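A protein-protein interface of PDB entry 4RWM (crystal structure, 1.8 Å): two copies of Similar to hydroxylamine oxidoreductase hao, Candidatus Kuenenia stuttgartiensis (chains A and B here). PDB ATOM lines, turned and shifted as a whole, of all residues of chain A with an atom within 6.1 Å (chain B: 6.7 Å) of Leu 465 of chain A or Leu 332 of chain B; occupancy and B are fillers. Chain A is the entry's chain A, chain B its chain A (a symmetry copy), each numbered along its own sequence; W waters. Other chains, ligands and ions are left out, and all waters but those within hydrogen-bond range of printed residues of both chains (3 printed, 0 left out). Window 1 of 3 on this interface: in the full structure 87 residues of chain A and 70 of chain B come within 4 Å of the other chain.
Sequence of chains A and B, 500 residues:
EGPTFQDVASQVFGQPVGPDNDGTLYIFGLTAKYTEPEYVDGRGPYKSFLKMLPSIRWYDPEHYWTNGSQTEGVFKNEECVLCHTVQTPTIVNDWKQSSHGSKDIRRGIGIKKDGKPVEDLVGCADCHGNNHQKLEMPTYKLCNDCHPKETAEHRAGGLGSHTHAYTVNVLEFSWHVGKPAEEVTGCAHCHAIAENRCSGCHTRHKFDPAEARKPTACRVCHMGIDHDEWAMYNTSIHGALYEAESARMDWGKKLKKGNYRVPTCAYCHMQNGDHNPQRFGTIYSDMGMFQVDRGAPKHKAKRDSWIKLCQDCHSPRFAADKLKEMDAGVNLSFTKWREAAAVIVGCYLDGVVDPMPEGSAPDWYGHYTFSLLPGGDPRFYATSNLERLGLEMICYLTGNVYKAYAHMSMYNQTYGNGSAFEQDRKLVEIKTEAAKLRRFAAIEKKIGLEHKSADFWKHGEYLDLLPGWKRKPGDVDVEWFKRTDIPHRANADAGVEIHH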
ATOM      1  N   ASP A  20      -9.404  -6.188  22.341  1.00  0.00           N
ATOM      2  CA  ASP A  20      -8.449  -5.093  22.194  1.00  0.00           C
ATOM      3  C   ASP A  20      -8.994  -3.742  22.675  1.00  0.00           C
ATOM      4  O   ASP A  20      -8.226  -2.899  23.141  1.00  0.00           O
ATOM      5  CB  ASP A  20      -7.932  -4.986  20.747  1.00  0.00           C
ATOM      6  CG  ASP A  20      -9.044  -4.802  19.708  1.00  0.00           C
ATOM      7  OD1 ASP A  20      -8.721  -4.866  18.504  1.00  0.00           O
ATOM      8  OD2 ASP A  20     -10.227  -4.600  20.066  1.00  0.00           O
ATOM      9  N   TYR A  34      -8.625  -9.049  18.231  1.00  0.00           N
ATOM     10  CA  TYR A  34      -9.071  -7.998  17.326  1.00  0.00           C
ATOM     11  C   TYR A  34     -10.591  -7.892  17.343  1.00  0.00           C
ATOM     12  O   TYR A  34     -11.295  -8.906  17.306  1.00  0.00           O
ATOM     13  CB  TYR A  34      -8.577  -8.255  15.901  1.00  0.00           C
ATOM     14  CG  TYR A  34      -9.186  -7.332  14.867  1.00  0.00           C
ATOM     15  CD1 TYR A  34      -8.703  -6.038  14.688  1.00  0.00           C
ATOM     16  CD2 TYR A  34     -10.245  -7.758  14.067  1.00  0.00           C
ATOM     17  CE1 TYR A  34      -9.265  -5.187  13.738  1.00  0.00           C
ATOM     18  CE2 TYR A  34     -10.814  -6.918  13.122  1.00  0.00           C
ATOM     19  CZ  TYR A  34     -10.322  -5.635  12.960  1.00  0.00           C
ATOM     20  OH  TYR A  34     -10.884  -4.808  12.015  1.00  0.00           O
ATOM     21  N   LYS A 179      -8.157  -3.556   1.696  1.00  0.00           N
ATOM     22  CA  LYS A 179      -7.724  -3.547   3.102  1.00  0.00           C
ATOM     23  C   LYS A 179      -8.838  -3.133   4.064  1.00  0.00           C
ATOM     24  O   LYS A 179      -9.769  -2.434   3.670  1.00  0.00           O
ATOM     25  CB  LYS A 179      -6.524  -2.608   3.268  1.00  0.00           C
ATOM     26  CG  LYS A 179      -5.246  -3.144   2.644  1.00  0.00           C
ATOM     27  CD  LYS A 179      -4.114  -2.132   2.719  1.00  0.00           C
ATOM     28  CE  LYS A 179      -2.766  -2.795   2.504  1.00  0.00           C
ATOM     29  NZ  LYS A 179      -2.383  -3.660   3.658  1.00  0.00           N
ATOM     30  N   PRO A 180      -8.744  -3.559   5.341  1.00  0.00           N
ATOM     31  CA  PRO A 180      -9.726  -3.103   6.328  1.00  0.00           C
ATOM     32  C   PRO A 180      -9.744  -1.582   6.426  1.00  0.00           C
ATOM     33  O   PRO A 180      -8.690  -0.948   6.363  1.00  0.00           O
ATOM     34  CB  PRO A 180      -9.232  -3.716   7.641  1.00  0.00           C
ATOM     35  CG  PRO A 180      -8.412  -4.873   7.242  1.00  0.00           C
ATOM     36  CD  PRO A 180      -7.795  -4.527   5.915  1.00  0.00           C
ATOM     37  N   GLU A 182     -10.097   0.810   8.652  1.00  0.00           N
ATOM     38  CA  GLU A 182      -9.314   1.575   9.639  1.00  0.00           C
ATOM     39  C   GLU A 182      -7.810   1.608   9.338  1.00  0.00           C
ATOM     40  O   GLU A 182      -7.090   2.454   9.871  1.00  0.00           O
ATOM     41  CB  GLU A 182      -9.553   1.067  11.068  1.00  0.00           C
ATOM     42  CG  GLU A 182      -8.968  -0.307  11.379  1.00  0.00           C
ATOM     43  CD  GLU A 182      -9.959  -1.439  11.215  1.00  0.00           C
ATOM     44  OE1 GLU A 182      -9.884  -2.393  12.017  1.00  0.00           O
ATOM     45  OE2 GLU A 182     -10.801  -1.378  10.292  1.00  0.00           O
ATOM     46  N   GLU A 183      -7.334   0.688   8.503  1.00  0.00           N
ATOM     47  CA  GLU A 183      -5.932   0.685   8.081  1.00  0.00           C
ATOM     48  C   GLU A 183      -5.597   1.820   7.107  1.00  0.00           C
ATOM     49  O   GLU A 183      -4.451   2.280   7.051  1.00  0.00           O
ATOM     50  CB  GLU A 183      -5.584  -0.655   7.430  1.00  0.00           C
ATOM     51  CG  GLU A 183      -4.117  -0.811   7.053  1.00  0.00           C
ATOM     52  CD  GLU A 183      -3.809  -2.137   6.391  1.00  0.00           C
ATOM     53  OE1 GLU A 183      -2.646  -2.334   5.992  1.00  0.00           O
ATOM     54  OE2 GLU A 183      -4.722  -2.981   6.264  1.00  0.00           O
ATOM     55  N   GLY A 460      -3.728 -16.113   8.759  1.00  0.00           N
ATOM     56  CA  GLY A 460      -3.172 -15.416   9.906  1.00  0.00           C
ATOM     57  C   GLY A 460      -4.170 -14.379  10.370  1.00  0.00           C
ATOM     58  O   GLY A 460      -5.150 -14.108   9.676  1.00  0.00           O
ATOM     59  N   GLU A 461      -3.930 -13.778  11.530  1.00  0.00           N
ATOM     60  CA  GLU A 461      -4.916 -12.866  12.111  1.00  0.00           C
ATOM     61  C   GLU A 461      -5.222 -11.677  11.207  1.00  0.00           C
ATOM     62  O   GLU A 461      -6.372 -11.249  11.137  1.00  0.00           O
ATOM     63  CB  GLU A 461      -4.483 -12.377  13.496  1.00  0.00           C
ATOM     64  CG  GLU A 461      -5.593 -11.627  14.229  1.00  0.00           C
ATOM     65  CD  GLU A 461      -5.221 -11.229  15.649  1.00  0.00           C
ATOM     66  OE1 GLU A 461      -4.147 -11.635  16.135  1.00  0.00           O
ATOM     67  OE2 GLU A 461      -6.015 -10.510  16.288  1.00  0.00           O
ATOM     68  N   TYR A 462      -4.204 -11.144  10.529  1.00  0.00           N
ATOM     69  CA  TYR A 462      -4.430 -10.054   9.579  1.00  0.00           C
ATOM     70  C   TYR A 462      -4.928 -10.582   8.233  1.00  0.00           C
ATOM     71  O   TYR A 462      -5.927 -10.088   7.702  1.00  0.00           O
ATOM     72  CB  TYR A 462      -3.177  -9.191   9.376  1.00  0.00           C
ATOM     73  CG  TYR A 462      -3.392  -8.140   8.309  1.00  0.00           C
ATOM     74  CD1 TYR A 462      -4.156  -7.006   8.567  1.00  0.00           C
ATOM     75  CD2 TYR A 462      -2.870  -8.307   7.028  1.00  0.00           C
ATOM     76  CE1 TYR A 462      -4.383  -6.052   7.583  1.00  0.00           C
ATOM     77  CE2 TYR A 462      -3.090  -7.359   6.035  1.00  0.00           C
ATOM     78  CZ  TYR A 462      -3.840  -6.238   6.316  1.00  0.00           C
ATOM     79  OH  TYR A 462      -4.047  -5.303   5.331  1.00  0.00           O
ATOM     80  N   LEU A 463      -4.242 -11.577   7.674  1.00  0.00           N
ATOM     81  CA  LEU A 463      -4.636 -12.114   6.357  1.00  0.00           C
ATOM     82  C   LEU A 463      -6.095 -12.557   6.323  1.00  0.00           C
ATOM     83  O   LEU A 463      -6.766 -12.391   5.303  1.00  0.00           O
ATOM     84  CB  LEU A 463      -3.741 -13.274   5.932  1.00  0.00           C
ATOM     85  CG  LEU A 463      -2.283 -12.949   5.627  1.00  0.00           C
ATOM     86  CD1 LEU A 463      -1.537 -14.225   5.253  1.00  0.00           C
ATOM     87  CD2 LEU A 463      -2.178 -11.905   4.517  1.00  0.00           C
ATOM     88  N   ASP A 464      -6.589 -13.096   7.438  1.00  0.00           N
ATOM     89  CA  ASP A 464      -7.979 -13.559   7.511  1.00  0.00           C
ATOM     90  C   ASP A 464      -9.009 -12.423   7.427  1.00  0.00           C
ATOM     91  O   ASP A 464     -10.185 -12.683   7.175  1.00  0.00           O
ATOM     92  CB  ASP A 464      -8.217 -14.378   8.791  1.00  0.00           C
ATOM     93  CG  ASP A 464      -7.481 -15.712   8.788  1.00  0.00           C
ATOM     94  OD1 ASP A 464      -7.513 -16.401   9.832  1.00  0.00           O
ATOM     95  OD2 ASP A 464      -6.859 -16.067   7.767  1.00  0.00           O
ATOM     96  N   LEU A 465      -8.575 -11.178   7.638  1.00  0.00           N
ATOM     97  CA  LEU A 465      -9.467 -10.012   7.549  1.00  0.00           C
ATOM     98  C   LEU A 465      -9.649  -9.487   6.127  1.00  0.00           C
ATOM     99  O   LEU A 465     -10.512  -8.640   5.891  1.00  0.00           O
ATOM    100  CB  LEU A 465      -8.937  -8.857   8.407  1.00  0.00           C
ATOM    101  CG  LEU A 465      -8.764  -9.100   9.904  1.00  0.00           C
ATOM    102  CD1 LEU A 465      -8.174  -7.854  10.554  1.00  0.00           C
ATOM    103  CD2 LEU A 465     -10.080  -9.469  10.570  1.00  0.00           C
ATOM    104  N   LEU A 466      -8.842  -9.968   5.186  1.00  0.00           N
ATOM    105  CA  LEU A 466      -8.823  -9.386   3.842  1.00  0.00           C
ATOM    106  C   LEU A 466     -10.107  -9.690   3.060  1.00  0.00           C
ATOM    107  O   LEU A 466     -10.693 -10.761   3.206  1.00  0.00           O
ATOM    108  CB  LEU A 466      -7.600  -9.871   3.067  1.00  0.00           C
ATOM    109  CG  LEU A 466      -6.246  -9.465   3.657  1.00  0.00           C
ATOM    110  CD1 LEU A 466      -5.097 -10.060   2.853  1.00  0.00           C
ATOM    111  CD2 LEU A 466      -6.125  -7.946   3.734  1.00  0.00           C
ATOM    112  N   PRO A 467     -10.541  -8.742   2.211  1.00  0.00           N
ATOM    113  CA  PRO A 467     -11.797  -8.859   1.471  1.00  0.00           C
ATOM    114  C   PRO A 467     -11.807  -9.929   0.370  1.00  0.00           C
ATOM    115  O   PRO A 467     -12.886 -10.367  -0.030  1.00  0.00           O
ATOM    116  CB  PRO A 467     -11.974  -7.458   0.872  1.00  0.00           C
ATOM    117  CG  PRO A 467     -10.598  -6.947   0.717  1.00  0.00           C
ATOM    118  CD  PRO A 467      -9.831  -7.493   1.884  1.00  0.00           C
ATOM    119  N   TRP A 469     -11.293 -13.008   0.535  1.00  0.00           N
ATOM    120  CA  TRP A 469     -12.030 -14.160   1.050  1.00  0.00           C
ATOM    121  C   TRP A 469     -13.544 -14.027   0.863  1.00  0.00           C
ATOM    122  O   TRP A 469     -14.233 -15.038   0.739  1.00  0.00           O
ATOM    123  CB  TRP A 469     -11.750 -14.361   2.547  1.00  0.00           C
ATOM    124  CG  TRP A 469     -10.319 -14.636   2.893  1.00  0.00           C
ATOM    125  CD1 TRP A 469      -9.461 -13.806   3.561  1.00  0.00           C
ATOM    126  CD2 TRP A 469      -9.581 -15.825   2.601  1.00  0.00           C
ATOM    127  NE1 TRP A 469      -8.233 -14.406   3.700  1.00  0.00           N
ATOM    128  CE2 TRP A 469      -8.279 -15.646   3.119  1.00  0.00           C
ATOM    129  CE3 TRP A 469      -9.892 -17.027   1.950  1.00  0.00           C
ATOM    130  CZ2 TRP A 469      -7.287 -16.623   3.003  1.00  0.00           C
ATOM    131  CZ3 TRP A 469      -8.911 -17.996   1.838  1.00  0.00           C
ATOM    132  CH2 TRP A 469      -7.623 -17.789   2.362  1.00  0.00           C
ATOM    133  N   LYS A 470     -14.043 -12.789   0.860  1.00  0.00           N
ATOM    134  CA  LYS A 470     -15.485 -12.493   0.841  1.00  0.00           C
ATOM    135  C   LYS A 470     -16.049 -12.272  -0.565  1.00  0.00           C
ATOM    136  O   LYS A 470     -17.265 -12.181  -0.722  1.00  0.00           O
ATOM    137  CB  LYS A 470     -15.797 -11.210   1.634  1.00  0.00           C
ATOM    138  CG  LYS A 470     -15.062 -11.001   2.964  1.00  0.00           C
ATOM    139  CD  LYS A 470     -15.436  -9.638   3.571  1.00  0.00           C
ATOM    140  CE  LYS A 470     -14.421  -9.151   4.604  1.00  0.00           C
ATOM    141  NZ  LYS A 470     -14.398  -9.978   5.837  1.00  0.00           N
ATOM    142  N   GLN B 291      -0.158  -2.672  23.667  1.00  0.00           N
ATOM    143  CA  GLN B 291      -1.413  -2.272  23.051  1.00  0.00           C
ATOM    144  C   GLN B 291      -2.405  -1.805  24.100  1.00  0.00           C
ATOM    145  O   GLN B 291      -2.675  -2.518  25.067  1.00  0.00           O
ATOM    146  CB  GLN B 291      -2.020  -3.442  22.273  1.00  0.00           C
ATOM    147  CG  GLN B 291      -3.325  -3.108  21.554  1.00  0.00           C
ATOM    148  CD  GLN B 291      -3.821  -4.248  20.679  1.00  0.00           C
ATOM    149  OE1 GLN B 291      -3.308  -5.367  20.747  1.00  0.00           O
ATOM    150  NE2 GLN B 291      -4.828  -3.967  19.852  1.00  0.00           N
ATOM    151  N   ASP B 327      -7.272   5.055  17.750  1.00  0.00           N
ATOM    152  CA  ASP B 327      -7.595   3.817  18.465  1.00  0.00           C
ATOM    153  C   ASP B 327      -7.782   2.667  17.479  1.00  0.00           C
ATOM    154  O   ASP B 327      -7.220   1.586  17.666  1.00  0.00           O
ATOM    155  CB  ASP B 327      -8.872   3.948  19.294  1.00  0.00           C
ATOM    156  CG  ASP B 327      -8.834   5.092  20.280  1.00  0.00           C
ATOM    157  OD1 ASP B 327      -7.745   5.407  20.806  1.00  0.00           O
ATOM    158  OD2 ASP B 327      -9.917   5.664  20.535  1.00  0.00           O
ATOM    159  N   ALA B 328      -8.569   2.907  16.431  1.00  0.00           N
ATOM    160  CA  ALA B 328      -8.860   1.873  15.434  1.00  0.00           C
ATOM    161  C   ALA B 328      -7.609   1.450  14.666  1.00  0.00           C
ATOM    162  O   ALA B 328      -7.372   0.261  14.467  1.00  0.00           O
ATOM    163  CB  ALA B 328      -9.944   2.353  14.457  1.00  0.00           C
ATOM    164  N   GLY B 329      -6.812   2.428  14.244  1.00  0.00           N
ATOM    165  CA  GLY B 329      -5.602   2.155  13.476  1.00  0.00           C
ATOM    166  C   GLY B 329      -4.569   1.391  14.275  1.00  0.00           C
ATOM    167  O   GLY B 329      -3.914   0.486  13.757  1.00  0.00           O
ATOM    168  N   VAL B 330      -4.424   1.761  15.543  1.00  0.00           N
ATOM    169  CA  VAL B 330      -3.535   1.048  16.452  1.00  0.00           C
ATOM    170  C   VAL B 330      -3.987  -0.411  16.605  1.00  0.00           C
ATOM    171  O   VAL B 330      -3.180  -1.332  16.486  1.00  0.00           O
ATOM    172  CB  VAL B 330      -3.444   1.747  17.829  1.00  0.00           C
ATOM    173  CG1 VAL B 330      -2.826   0.817  18.881  1.00  0.00           C
ATOM    174  CG2 VAL B 330      -2.627   3.033  17.713  1.00  0.00           C
ATOM    175  N   ASN B 331      -5.276  -0.630  16.834  1.00  0.00           N
ATOM    176  CA  ASN B 331      -5.758  -1.995  17.058  1.00  0.00           C
ATOM    177  C   ASN B 331      -5.569  -2.892  15.835  1.00  0.00           C
ATOM    178  O   ASN B 331      -5.242  -4.072  15.972  1.00  0.00           O
ATOM    179  CB  ASN B 331      -7.214  -1.991  17.529  1.00  0.00           C
ATOM    180  CG  ASN B 331      -7.373  -1.465  18.952  1.00  0.00           C
ATOM    181  OD1 ASN B 331      -6.416  -1.435  19.733  1.00  0.00           O
ATOM    182  ND2 ASN B 331      -8.590  -1.060  19.298  1.00  0.00           N
ATOM    183  N   LEU B 332      -5.747  -2.339  14.639  1.00  0.00           N
ATOM    184  CA  LEU B 332      -5.501  -3.105  13.412  1.00  0.00           C
ATOM    185  C   LEU B 332      -4.010  -3.453  13.294  1.00  0.00           C
ATOM    186  O   LEU B 332      -3.652  -4.583  12.942  1.00  0.00           O
ATOM    187  CB  LEU B 332      -6.004  -2.326  12.189  1.00  0.00           C
ATOM    188  CG  LEU B 332      -5.998  -2.991  10.801  1.00  0.00           C
ATOM    189  CD1 LEU B 332      -4.594  -3.061  10.217  1.00  0.00           C
ATOM    190  CD2 LEU B 332      -6.639  -4.380  10.823  1.00  0.00           C
ATOM    191  N   SER B 333      -3.143  -2.496  13.636  1.00  0.00           N
ATOM    192  CA  SER B 333      -1.693  -2.687  13.530  1.00  0.00           C
ATOM    193  C   SER B 333      -1.177  -3.881  14.338  1.00  0.00           C
ATOM    194  O   SER B 333      -0.217  -4.534  13.936  1.00  0.00           O
ATOM    195  CB  SER B 333      -0.930  -1.414  13.939  1.00  0.00           C
ATOM    196  OG  SER B 333      -0.848  -1.259  15.348  1.00  0.00           O
ATOM    197  N   PHE B 334      -1.816  -4.173  15.466  1.00  0.00           N
ATOM    198  CA  PHE B 334      -1.370  -5.283  16.305  1.00  0.00           C
ATOM    199  C   PHE B 334      -1.703  -6.667  15.746  1.00  0.00           C
ATOM    200  O   PHE B 334      -1.078  -7.645  16.153  1.00  0.00           O
ATOM    201  CB  PHE B 334      -1.868  -5.127  17.741  1.00  0.00           C
ATOM    202  CG  PHE B 334      -0.952  -4.297  18.586  1.00  0.00           C
ATOM    203  CD1 PHE B 334       0.128  -4.880  19.219  1.00  0.00           C
ATOM    204  CD2 PHE B 334      -1.137  -2.927  18.707  1.00  0.00           C
ATOM    205  CE1 PHE B 334       0.998  -4.126  19.978  1.00  0.00           C
ATOM    206  CE2 PHE B 334      -0.270  -2.160  19.480  1.00  0.00           C
ATOM    207  CZ  PHE B 334       0.798  -2.761  20.111  1.00  0.00           C
ATOM    208  N   THR B 335      -2.649  -6.753  14.808  1.00  0.00           N
ATOM    209  CA  THR B 335      -2.928  -8.035  14.144  1.00  0.00           C
ATOM    210  C   THR B 335      -1.708  -8.514  13.359  1.00  0.00           C
ATOM    211  O   THR B 335      -1.400  -9.706  13.338  1.00  0.00           O
ATOM    212  CB  THR B 335      -4.165  -7.972  13.207  1.00  0.00           C
ATOM    213  OG1 THR B 335      -3.924  -7.073  12.112  1.00  0.00           O
ATOM    214  CG2 THR B 335      -5.403  -7.532  13.977  1.00  0.00           C
ATOM    215  N   LYS B 336      -0.998  -7.571  12.743  1.00  0.00           N
ATOM    216  CA  LYS B 336       0.181  -7.888  11.951  1.00  0.00           C
ATOM    217  C   LYS B 336       1.360  -8.274  12.843  1.00  0.00           C
ATOM    218  O   LYS B 336       2.135  -9.172  12.499  1.00  0.00           O
ATOM    219  CB  LYS B 336       0.557  -6.705  11.059  1.00  0.00           C
ATOM    220  CG  LYS B 336      -0.526  -6.307  10.070  1.00  0.00           C
ATOM    221  CD  LYS B 336      -0.134  -5.035   9.330  1.00  0.00           C
ATOM    222  CE  LYS B 336      -1.267  -4.499   8.470  1.00  0.00           C
ATOM    223  NZ  LYS B 336      -0.896  -3.197   7.825  1.00  0.00           N
ATOM    224  N   TRP B 337       1.492  -7.608  13.988  1.00  0.00           N
ATOM    225  CA  TRP B 337       2.534  -7.965  14.949  1.00  0.00           C
ATOM    226  C   TRP B 337       2.295  -9.376  15.505  1.00  0.00           C
ATOM    227  O   TRP B 337       3.226 -10.177  15.605  1.00  0.00           O
ATOM    228  CB  TRP B 337       2.627  -6.929  16.079  1.00  0.00           C
ATOM    229  CG  TRP B 337       3.315  -7.435  17.315  1.00  0.00           C
ATOM    230  CD1 TRP B 337       2.787  -7.488  18.570  1.00  0.00           C
ATOM    231  CD2 TRP B 337       4.641  -7.978  17.413  1.00  0.00           C
ATOM    232  NE1 TRP B 337       3.699  -8.024  19.447  1.00  0.00           N
ATOM    233  CE2 TRP B 337       4.844  -8.335  18.763  1.00  0.00           C
ATOM    234  CE3 TRP B 337       5.677  -8.196  16.493  1.00  0.00           C
ATOM    235  CZ2 TRP B 337       6.043  -8.892  19.219  1.00  0.00           C
ATOM    236  CZ3 TRP B 337       6.864  -8.759  16.946  1.00  0.00           C
ATOM    237  CH2 TRP B 337       7.036  -9.100  18.300  1.00  0.00           C
ATOM    238  N   ARG B 338       1.050  -9.680  15.856  1.00  0.00           N
ATOM    239  CA  ARG B 338       0.725 -11.000  16.396  1.00  0.00           C
ATOM    240  C   ARG B 338       0.979 -12.095  15.359  1.00  0.00           C
ATOM    241  O   ARG B 338       1.476 -13.162  15.707  1.00  0.00           O
ATOM    242  CB  ARG B 338      -0.705 -11.052  16.950  1.00  0.00           C
ATOM    243  CG  ARG B 338      -0.849 -10.368  18.311  1.00  0.00           C
ATOM    244  CD  ARG B 338      -2.201 -10.626  18.955  1.00  0.00           C
ATOM    245  NE  ARG B 338      -3.301  -9.982  18.235  1.00  0.00           N
ATOM    246  CZ  ARG B 338      -3.746  -8.741  18.451  1.00  0.00           C
ATOM    247  NH1 ARG B 338      -3.204  -7.961  19.388  1.00  0.00           N
ATOM    248  NH2 ARG B 338      -4.756  -8.280  17.726  1.00  0.00           N
ATOM    249  N   ALA B 420       1.438   1.333   8.370  1.00  0.00           N
ATOM    250  CA  ALA B 420       0.749   0.079   8.073  1.00  0.00           C
ATOM    251  C   ALA B 420       1.427  -0.683   6.938  1.00  0.00           C
ATOM    252  O   ALA B 420       1.609  -1.891   7.023  1.00  0.00           O
ATOM    253  CB  ALA B 420      -0.705   0.352   7.707  1.00  0.00           C
ATOM    254  N   GLN B 423       4.716  -2.136   7.882  1.00  0.00           N
ATOM    255  CA  GLN B 423       4.404  -3.372   8.622  1.00  0.00           C
ATOM    256  C   GLN B 423       4.153  -4.540   7.674  1.00  0.00           C
ATOM    257  O   GLN B 423       4.654  -5.644   7.901  1.00  0.00           O
ATOM    258  CB  GLN B 423       3.164  -3.211   9.505  1.00  0.00           C
ATOM    259  CG  GLN B 423       3.383  -2.521  10.829  1.00  0.00           C
ATOM    260  CD  GLN B 423       2.132  -2.593  11.685  1.00  0.00           C
ATOM    261  OE1 GLN B 423       1.067  -2.148  11.267  1.00  0.00           O
ATOM    262  NE2 GLN B 423       2.247  -3.182  12.868  1.00  0.00           N
HETATM  263  O   HOH W   1      -9.259  -1.787  14.600  1.00  0.00           O
HETATM  264  O   HOH W   2      -6.160  -5.682  17.954  1.00  0.00           O
HETATM  265  O   HOH W   3     -10.365  -2.669  16.879  1.00  0.00           O
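OE1 of Gln 291 of chain B lies within hydrogen-bond range of NH1 of Arg 338 of chain B (2.9 Å). The side-chain hydroxyl (OH) of Tyr 34 of chain A is in hydrogen-bond range of the side-chain carboxylate (OE1) of Glu 182 of chain A, at 2.6 Å. The side-chain amino group (NZ) of Lys 179 of chain A sits at hydrogen-bond distance from the side-chain hydroxyl (OH) of Tyr 462 of chain A (2.9 Å). The side-chain amide oxygen (OD1) of Asn 331 of chain B is in hydrogen-bond range of the side-chain amide nitrogen (NE2) of Gln 291 of chain B (3.0 Å). The side-chain amino group (NZ) of Lys 179 of chain A is in salt-bridge range of the side-chain carboxylate (OE1) of Glu 183 of chain A, 2.7 Å away. The backbone carbonyl oxygen (O) of Ala 420 of chain B is in hydrogen-bond range of the side-chain amino group (NZ) of Lys 336 of chain B (2.9 Å).
No position is printed for both chains. Of the 16 pairs that touch across the chains among the printed residues, none has its exchanged pair printed and touching as well.
Of the 16 printed residues of chain A, 7 touch a printed residue of chain B. Printed residues of chain A that touch a printed residue of chain B: Asp 20, Tyr 34, Glu 182, Glu 183, Glu 461, Tyr 462 and Leu 465. Hydrophobic or aromatic side chains of chain B within 4 Å of the printed part of chain A: Ala 328, Leu 332 and Ala 420. Among the printed residues, 16 pairs touch across the chains. Among the printed residues, Asp or Glu carboxylates within 4 Å of a Lys or Arg side-chain nitrogen of the other chain: Glu 183 of chain A with Lys 336 of chain B (2.7 Å) and Glu 461 of chain A with Arg 338 of chain B (2.8 Å).
Of the printed residues of chain B, Glu 461 of chain A touches Thr 335 (3.8 Å) and Arg 338 (2.8 Å). Leu 465 of chain A touches just one residue of chain B: Leu 332 (3.8 Å). Printed residues of chain A within 4 Å of Leu 332 of chain B: Glu 182, Glu 183, Tyr 462 and Leu 465. Printed residues of chain A within 4 Å of Lys 336 of chain B: Glu 183 (2.7 Å) and Tyr 462 (3.6 Å). The nearest residue of chain B that does not touch Leu 465 of chain A is Thr 335 of chain B (4.4 Å). The nearest printed residue of chain A that does not touch Leu 332 of chain B is Tyr 34 of chain A (4.01 Å). The nearest printed residue of chain A that does not touch Ala 420 of chain B is Lys 179 of chain A (5.5 Å).
Water W2 lies within hydrogen-bond range of the backbone carbonyl oxygen of Asn 331 of chain B (2.7 Å), the side-chain carboxylate of Asp 20 of chain A (2.7 Å), the side-chain amide nitrogen of Gln 291 of chain B (2.9 Å) and the guanidinium group of Arg 338 of chain B (3.0 Å). Water W1 lies within hydrogen-bond range of OE1 of Glu 182 of chain A and O of Ala 328 of chain B. Water W3 bridges OD1 of Asp 20 of chain A (3.2 Å) and ND2 of Asn 331 of chain B (3.4 Å).
Among the printed residues, merely in contact across the chains: Asp 20 of chain A with Gln 291 of chain B, Asp 20 of chain A with Asn 331 of chain B, Glu 182 of chain A with Ala 328 of chain B, Tyr 462 of chain A with Thr 335 of chain B, Tyr 462 of chain A with Lys 336 of chain B, Glu 183 of chain A with Ala 420 of chain B, Glu 182 of chain A with Leu 332 of chain B, Tyr 34 of chain A with Thr 335 of chain B, Leu 465 of chain A with Leu 332 of chain B, Glu 183 of chain A with Leu 332 of chain B, Glu 461 of chain A with Thr 335 of chain B, Glu 182 of chain A with Gly 329 of chain B, Tyr 34 of chain A with Arg 338 of chain B and Tyr 462 of chain A with Leu 332 of chain B.
OE1 of Glu 461 of chain A is in salt-bridge range of NE of Arg 338 of chain B. The side-chain amino group of Lys 336 of chain B lies within salt-bridge range of the side-chain carboxylate of Glu 183 of chain A.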
